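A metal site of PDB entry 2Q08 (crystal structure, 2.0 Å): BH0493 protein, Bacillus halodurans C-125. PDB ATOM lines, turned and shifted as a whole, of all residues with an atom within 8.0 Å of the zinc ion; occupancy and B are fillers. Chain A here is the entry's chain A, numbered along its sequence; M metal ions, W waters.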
ATOM      1  N   HIS A  26      27.187  17.126  -3.464  1.00  0.00           N
ATOM      2  CA  HIS A  26      27.044  16.818  -2.042  1.00  0.00           C
ATOM      3  C   HIS A  26      27.242  15.343  -1.738  1.00  0.00           C
ATOM      4  O   HIS A  26      26.411  14.502  -2.096  1.00  0.00           O
ATOM      5  CB  HIS A  26      25.707  17.245  -1.475  1.00  0.00           C
ATOM      6  CG  HIS A  26      25.569  16.921  -0.013  1.00  0.00           C
ATOM      7  ND1 HIS A  26      26.403  17.451   0.938  1.00  0.00           N
ATOM      8  CD2 HIS A  26      24.754  16.058   0.629  1.00  0.00           C
ATOM      9  CE1 HIS A  26      26.112  16.935   2.120  1.00  0.00           C
ATOM     10  NE2 HIS A  26      25.118  16.085   1.959  1.00  0.00           N
ATOM     11  N   THR A  27      28.363  15.037  -1.079  1.00  0.00           N
ATOM     12  CA  THR A  27      28.704  13.663  -0.733  1.00  0.00           C
ATOM     13  C   THR A  27      29.405  13.650   0.617  1.00  0.00           C
ATOM     14  O   THR A  27      29.672  14.693   1.210  1.00  0.00           O
ATOM     15  CB  THR A  27      29.681  13.029  -1.741  1.00  0.00           C
ATOM     16  OG1 THR A  27      31.005  13.547  -1.516  1.00  0.00           O
ATOM     17  CG2 THR A  27      29.273  13.338  -3.171  1.00  0.00           C
ATOM     18  N   HIS A  28      29.709  12.447   1.079  1.00  0.00           N
ATOM     19  CA  HIS A  28      30.415  12.247   2.333  1.00  0.00           C
ATOM     20  C   HIS A  28      31.684  11.470   2.003  1.00  0.00           C
ATOM     21  O   HIS A  28      32.113  10.596   2.762  1.00  0.00           O
ATOM     22  CB  HIS A  28      29.547  11.476   3.315  1.00  0.00           C
ATOM     23  CG  HIS A  28      28.463  12.315   3.930  1.00  0.00           C
ATOM     24  ND1 HIS A  28      28.706  13.194   4.963  1.00  0.00           N
ATOM     25  CD2 HIS A  28      27.160  12.448   3.613  1.00  0.00           C
ATOM     26  CE1 HIS A  28      27.596  13.830   5.264  1.00  0.00           C
ATOM     27  NE2 HIS A  28      26.644  13.402   4.463  1.00  0.00           N
ATOM     28  N   HIS A  49      24.676   2.606   6.613  1.00  0.00           N
ATOM     29  CA  HIS A  49      23.597   2.677   7.593  1.00  0.00           C
ATOM     30  C   HIS A  49      22.205   2.419   7.040  1.00  0.00           C
ATOM     31  O   HIS A  49      21.311   2.008   7.776  1.00  0.00           O
ATOM     32  CB  HIS A  49      23.674   3.992   8.388  1.00  0.00           C
ATOM     33  CG  HIS A  49      23.276   5.214   7.623  1.00  0.00           C
ATOM     34  ND1 HIS A  49      21.970   5.661   7.546  1.00  0.00           N
ATOM     35  CD2 HIS A  49      24.022   6.124   6.940  1.00  0.00           C
ATOM     36  CE1 HIS A  49      21.929   6.785   6.863  1.00  0.00           C
ATOM     37  NE2 HIS A  49      23.159   7.086   6.480  1.00  0.00           N
ATOM     38  N   TYR A  50      22.007   2.634   5.733  1.00  0.00           N
ATOM     39  CA  TYR A  50      20.697   2.383   5.129  1.00  0.00           C
ATOM     40  C   TYR A  50      20.379   0.892   5.300  1.00  0.00           C
ATOM     41  O   TYR A  50      19.244   0.524   5.590  1.00  0.00           O
ATOM     42  CB  TYR A  50      20.711   2.700   3.633  1.00  0.00           C
ATOM     43  CG  TYR A  50      20.578   4.169   3.254  1.00  0.00           C
ATOM     44  CD1 TYR A  50      21.209   5.169   3.996  1.00  0.00           C
ATOM     45  CD2 TYR A  50      19.888   4.541   2.094  1.00  0.00           C
ATOM     46  CE1 TYR A  50      21.161   6.513   3.586  1.00  0.00           C
ATOM     47  CE2 TYR A  50      19.839   5.887   1.671  1.00  0.00           C
ATOM     48  CZ  TYR A  50      20.481   6.858   2.421  1.00  0.00           C
ATOM     49  OH  TYR A  50      20.453   8.168   1.999  1.00  0.00           O
ATOM     50  N   THR A 143      31.960  16.763   2.392  1.00  0.00           N
ATOM     51  CA  THR A 143      31.316  17.355   3.549  1.00  0.00           C
ATOM     52  C   THR A 143      32.476  17.424   4.550  1.00  0.00           C
ATOM     53  O   THR A 143      32.886  16.412   5.128  1.00  0.00           O
ATOM     54  CB  THR A 143      30.201  16.457   4.122  1.00  0.00           C
ATOM     55  OG1 THR A 143      29.117  16.382   3.190  1.00  0.00           O
ATOM     56  CG2 THR A 143      29.692  17.014   5.449  1.00  0.00           C
ATOM     57  N   ARG A 170      30.960  22.225   6.731  1.00  0.00           N
ATOM     58  CA  ARG A 170      29.836  21.758   7.542  1.00  0.00           C
ATOM     59  C   ARG A 170      29.829  22.465   8.896  1.00  0.00           C
ATOM     60  O   ARG A 170      30.815  22.396   9.641  1.00  0.00           O
ATOM     61  CB  ARG A 170      29.922  20.248   7.750  1.00  0.00           C
ATOM     62  CG  ARG A 170      28.832  19.641   8.622  1.00  0.00           C
ATOM     63  CD  ARG A 170      29.023  18.141   8.757  1.00  0.00           C
ATOM     64  NE  ARG A 170      28.009  17.494   9.592  1.00  0.00           N
ATOM     65  CZ  ARG A 170      27.945  17.601  10.910  1.00  0.00           C
ATOM     66  NH1 ARG A 170      28.835  18.333  11.578  1.00  0.00           N
ATOM     67  NH2 ARG A 170      26.983  16.970  11.581  1.00  0.00           N
ATOM     68  N   TYR A 219      30.624  26.053  -0.646  1.00  0.00           N
ATOM     69  CA  TYR A 219      29.480  26.528   0.117  1.00  0.00           C
ATOM     70  C   TYR A 219      29.568  26.082   1.582  1.00  0.00           C
ATOM     71  O   TYR A 219      30.340  25.175   1.910  1.00  0.00           O
ATOM     72  CB  TYR A 219      28.139  26.052  -0.503  1.00  0.00           C
ATOM     73  CG  TYR A 219      27.930  24.551  -0.530  1.00  0.00           C
ATOM     74  CD1 TYR A 219      27.668  23.833   0.632  1.00  0.00           C
ATOM     75  CD2 TYR A 219      28.003  23.853  -1.741  1.00  0.00           C
ATOM     76  CE1 TYR A 219      27.480  22.439   0.594  1.00  0.00           C
ATOM     77  CE2 TYR A 219      27.818  22.472  -1.784  1.00  0.00           C
ATOM     78  CZ  TYR A 219      27.550  21.773  -0.618  1.00  0.00           C
ATOM     79  OH  TYR A 219      27.384  20.402  -0.682  1.00  0.00           O
ATOM     80  N   SER A 223      22.471  20.894   8.440  1.00  0.00           N
ATOM     81  CA  SER A 223      21.261  20.100   8.293  1.00  0.00           C
ATOM     82  C   SER A 223      20.396  20.576   9.458  1.00  0.00           C
ATOM     83  O   SER A 223      20.883  20.740  10.578  1.00  0.00           O
ATOM     84  CB  SER A 223      21.567  18.601   8.361  1.00  0.00           C
ATOM     85  OG  SER A 223      21.947  18.236   9.674  1.00  0.00           O
ATOM     86  N   MET A 258      19.938  21.733   4.587  1.00  0.00           N
ATOM     87  CA  MET A 258      19.327  20.439   4.376  1.00  0.00           C
ATOM     88  C   MET A 258      18.339  20.305   5.541  1.00  0.00           C
ATOM     89  O   MET A 258      18.721  19.975   6.666  1.00  0.00           O
ATOM     90  CB  MET A 258      20.395  19.353   4.386  1.00  0.00           C
ATOM     91  CG  MET A 258      21.566  19.725   3.479  1.00  0.00           C
ATOM     92  SD  MET A 258      22.631  18.364   3.027  1.00  0.00           S
ATOM     93  CE  MET A 258      23.544  18.128   4.549  1.00  0.00           C
ATOM     94  N   THR A 299      17.660  21.584   0.136  1.00  0.00           N
ATOM     95  CA  THR A 299      17.114  20.264  -0.159  1.00  0.00           C
ATOM     96  C   THR A 299      16.325  19.928   1.102  1.00  0.00           C
ATOM     97  O   THR A 299      16.728  20.301   2.210  1.00  0.00           O
ATOM     98  CB  THR A 299      18.209  19.200  -0.455  1.00  0.00           C
ATOM     99  OG1 THR A 299      17.612  18.077  -1.110  1.00  0.00           O
ATOM    100  CG2 THR A 299      18.883  18.713   0.823  1.00  0.00           C
ATOM    101  N   PHE A 322      18.249  21.412  -4.801  1.00  0.00           N
ATOM    102  CA  PHE A 322      19.045  20.317  -5.309  1.00  0.00           C
ATOM    103  C   PHE A 322      18.721  18.964  -4.712  1.00  0.00           C
ATOM    104  O   PHE A 322      18.363  18.858  -3.537  1.00  0.00           O
ATOM    105  CB  PHE A 322      20.540  20.593  -5.064  1.00  0.00           C
ATOM    106  CG  PHE A 322      20.942  20.482  -3.608  1.00  0.00           C
ATOM    107  CD1 PHE A 322      21.464  19.299  -3.105  1.00  0.00           C
ATOM    108  CD2 PHE A 322      20.811  21.577  -2.744  1.00  0.00           C
ATOM    109  CE1 PHE A 322      21.847  19.189  -1.756  1.00  0.00           C
ATOM    110  CE2 PHE A 322      21.187  21.486  -1.392  1.00  0.00           C
ATOM    111  CZ  PHE A 322      21.709  20.282  -0.900  1.00  0.00           C
ATOM    112  N   TRP A 325      17.174  13.960  -1.453  1.00  0.00           N
ATOM    113  CA  TRP A 325      17.892  13.590  -0.250  1.00  0.00           C
ATOM    114  C   TRP A 325      17.380  12.435   0.600  1.00  0.00           C
ATOM    115  O   TRP A 325      16.202  12.385   0.959  1.00  0.00           O
ATOM    116  CB  TRP A 325      18.027  14.863   0.594  1.00  0.00           C
ATOM    117  CG  TRP A 325      18.811  14.757   1.854  1.00  0.00           C
ATOM    118  CD1 TRP A 325      19.971  14.060   2.057  1.00  0.00           C
ATOM    119  CD2 TRP A 325      18.548  15.457   3.077  1.00  0.00           C
ATOM    120  NE1 TRP A 325      20.444  14.289   3.332  1.00  0.00           N
ATOM    121  CE2 TRP A 325      19.594  15.145   3.973  1.00  0.00           C
ATOM    122  CE3 TRP A 325      17.533  16.334   3.496  1.00  0.00           C
ATOM    123  CZ2 TRP A 325      19.649  15.669   5.273  1.00  0.00           C
ATOM    124  CZ3 TRP A 325      17.588  16.860   4.782  1.00  0.00           C
ATOM    125  CH2 TRP A 325      18.644  16.523   5.659  1.00  0.00           C
ATOM    126  N   TRP A 326      18.269  11.484   0.868  1.00  0.00           N
ATOM    127  CA  TRP A 326      17.994  10.375   1.777  1.00  0.00           C
ATOM    128  C   TRP A 326      16.701   9.591   1.527  1.00  0.00           C
ATOM    129  O   TRP A 326      16.624   8.761   0.620  1.00  0.00           O
ATOM    130  CB  TRP A 326      17.964  10.976   3.186  1.00  0.00           C
ATOM    131  CG  TRP A 326      18.321  10.095   4.318  1.00  0.00           C
ATOM    132  CD1 TRP A 326      18.238   8.732   4.383  1.00  0.00           C
ATOM    133  CD2 TRP A 326      18.748  10.530   5.615  1.00  0.00           C
ATOM    134  NE1 TRP A 326      18.588   8.291   5.641  1.00  0.00           N
ATOM    135  CE2 TRP A 326      18.908   9.376   6.412  1.00  0.00           C
ATOM    136  CE3 TRP A 326      19.013  11.785   6.173  1.00  0.00           C
ATOM    137  CZ2 TRP A 326      19.315   9.450   7.749  1.00  0.00           C
ATOM    138  CZ3 TRP A 326      19.420  11.859   7.509  1.00  0.00           C
ATOM    139  CH2 TRP A 326      19.570  10.695   8.276  1.00  0.00           C
ATOM    140  N   HIS A 353      22.101  14.546  -6.296  1.00  0.00           N
ATOM    141  CA  HIS A 353      23.411  14.483  -5.637  1.00  0.00           C
ATOM    142  C   HIS A 353      23.388  13.071  -5.051  1.00  0.00           C
ATOM    143  O   HIS A 353      22.318  12.513  -4.831  1.00  0.00           O
ATOM    144  CB  HIS A 353      23.596  15.560  -4.555  1.00  0.00           C
ATOM    145  CG  HIS A 353      22.698  15.403  -3.375  1.00  0.00           C
ATOM    146  ND1 HIS A 353      21.421  15.904  -3.336  1.00  0.00           N
ATOM    147  CD2 HIS A 353      22.903  14.809  -2.175  1.00  0.00           C
ATOM    148  CE1 HIS A 353      20.875  15.631  -2.162  1.00  0.00           C
ATOM    149  NE2 HIS A 353      21.757  14.963  -1.438  1.00  0.00           N
ATOM    150  N   SER A 354      24.564  12.471  -4.810  1.00  0.00           N
ATOM    151  CA  SER A 354      24.611  11.100  -4.312  1.00  0.00           C
ATOM    152  C   SER A 354      24.589  10.950  -2.795  1.00  0.00           C
ATOM    153  O   SER A 354      24.030   9.975  -2.264  1.00  0.00           O
ATOM    154  CB  SER A 354      25.868  10.392  -4.809  1.00  0.00           C
ATOM    155  OG  SER A 354      26.998  10.837  -4.096  1.00  0.00           O
ATOM    156  N   ASP A 355      25.200  11.885  -2.092  1.00  0.00           N
ATOM    157  CA  ASP A 355      25.265  11.792  -0.653  1.00  0.00           C
ATOM    158  C   ASP A 355      26.037  10.513  -0.302  1.00  0.00           C
ATOM    159  O   ASP A 355      25.868   9.942   0.775  1.00  0.00           O
ATOM    160  CB  ASP A 355      23.852  11.703  -0.079  1.00  0.00           C
ATOM    161  CG  ASP A 355      23.669  12.555   1.125  1.00  0.00           C
ATOM    162  OD1 ASP A 355      24.467  12.423   2.072  1.00  0.00           O
ATOM    163  OD2 ASP A 355      22.722  13.370   1.130  1.00  0.00           O
ATOM    164  N   ALA A 356      26.867  10.049  -1.242  1.00  0.00           N
ATOM    165  CA  ALA A 356      27.626   8.821  -1.025  1.00  0.00           C
ATOM    166  C   ALA A 356      28.508   8.861   0.229  1.00  0.00           C
ATOM    167  O   ALA A 356      29.191   9.848   0.493  1.00  0.00           O
ATOM    168  CB  ALA A 356      28.486   8.530  -2.259  1.00  0.00           C
ATOM    169  N   ARG A 357      28.476   7.782   0.987  1.00  0.00           N
ATOM    170  CA  ARG A 357      29.283   7.662   2.187  1.00  0.00           C
ATOM    171  C   ARG A 357      30.383   6.663   1.902  1.00  0.00           C
ATOM    172  O   ARG A 357      31.441   6.673   2.537  1.00  0.00           O
ATOM    173  CB  ARG A 357      28.448   7.172   3.366  1.00  0.00           C
ATOM    174  CG  ARG A 357      27.638   8.267   4.025  1.00  0.00           C
ATOM    175  CD  ARG A 357      26.803   7.736   5.183  1.00  0.00           C
ATOM    176  NE  ARG A 357      26.182   8.824   5.915  1.00  0.00           N
ATOM    177  CZ  ARG A 357      26.851   9.725   6.625  1.00  0.00           C
ATOM    178  NH1 ARG A 357      28.174   9.664   6.702  1.00  0.00           N
ATOM    179  NH2 ARG A 357      26.206  10.702   7.259  1.00  0.00           N
HETATM  180 ZN    ZN M   1      24.583  14.298   3.384  1.00  0.00          ZN
HETATM  181  O   HOH W   1      23.661  14.833   5.120  1.00  0.00           O
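Water W1 is bound to the zinc ion (2.0 Å).
The side-chain carboxylate (OD1) of Asp 355 is bound to the zinc ion (2.3 Å).
NE2 of His 26 is bound to the zinc ion, 2.3 Å away.
NE2 of His 28 binds the zinc ion, 2.5 Å away.
The zinc ion has four donor atoms within binding distance.
SD of Met 258 sits close to NE2 of His 26 (3.5 Å).
A ring nitrogen (NE2) of His 353 sits at hydrogen-bond distance from the side-chain carboxylate of Asp 355 (3.2 Å).
The backbone carbonyl oxygen (O) of Ala 356 sits at hydrogen-bond distance from the backbone NH (N) of His 28.
The side-chain carboxylate (OD2) of Asp 355 sits close to the indole nitrogen (NE1) of Trp 325.
Of the 19 residues printed, 3 come within 4 Å of the zinc ion.
The nearest printed residue that does not touch the zinc ion is Met 258 (4.1 Å).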
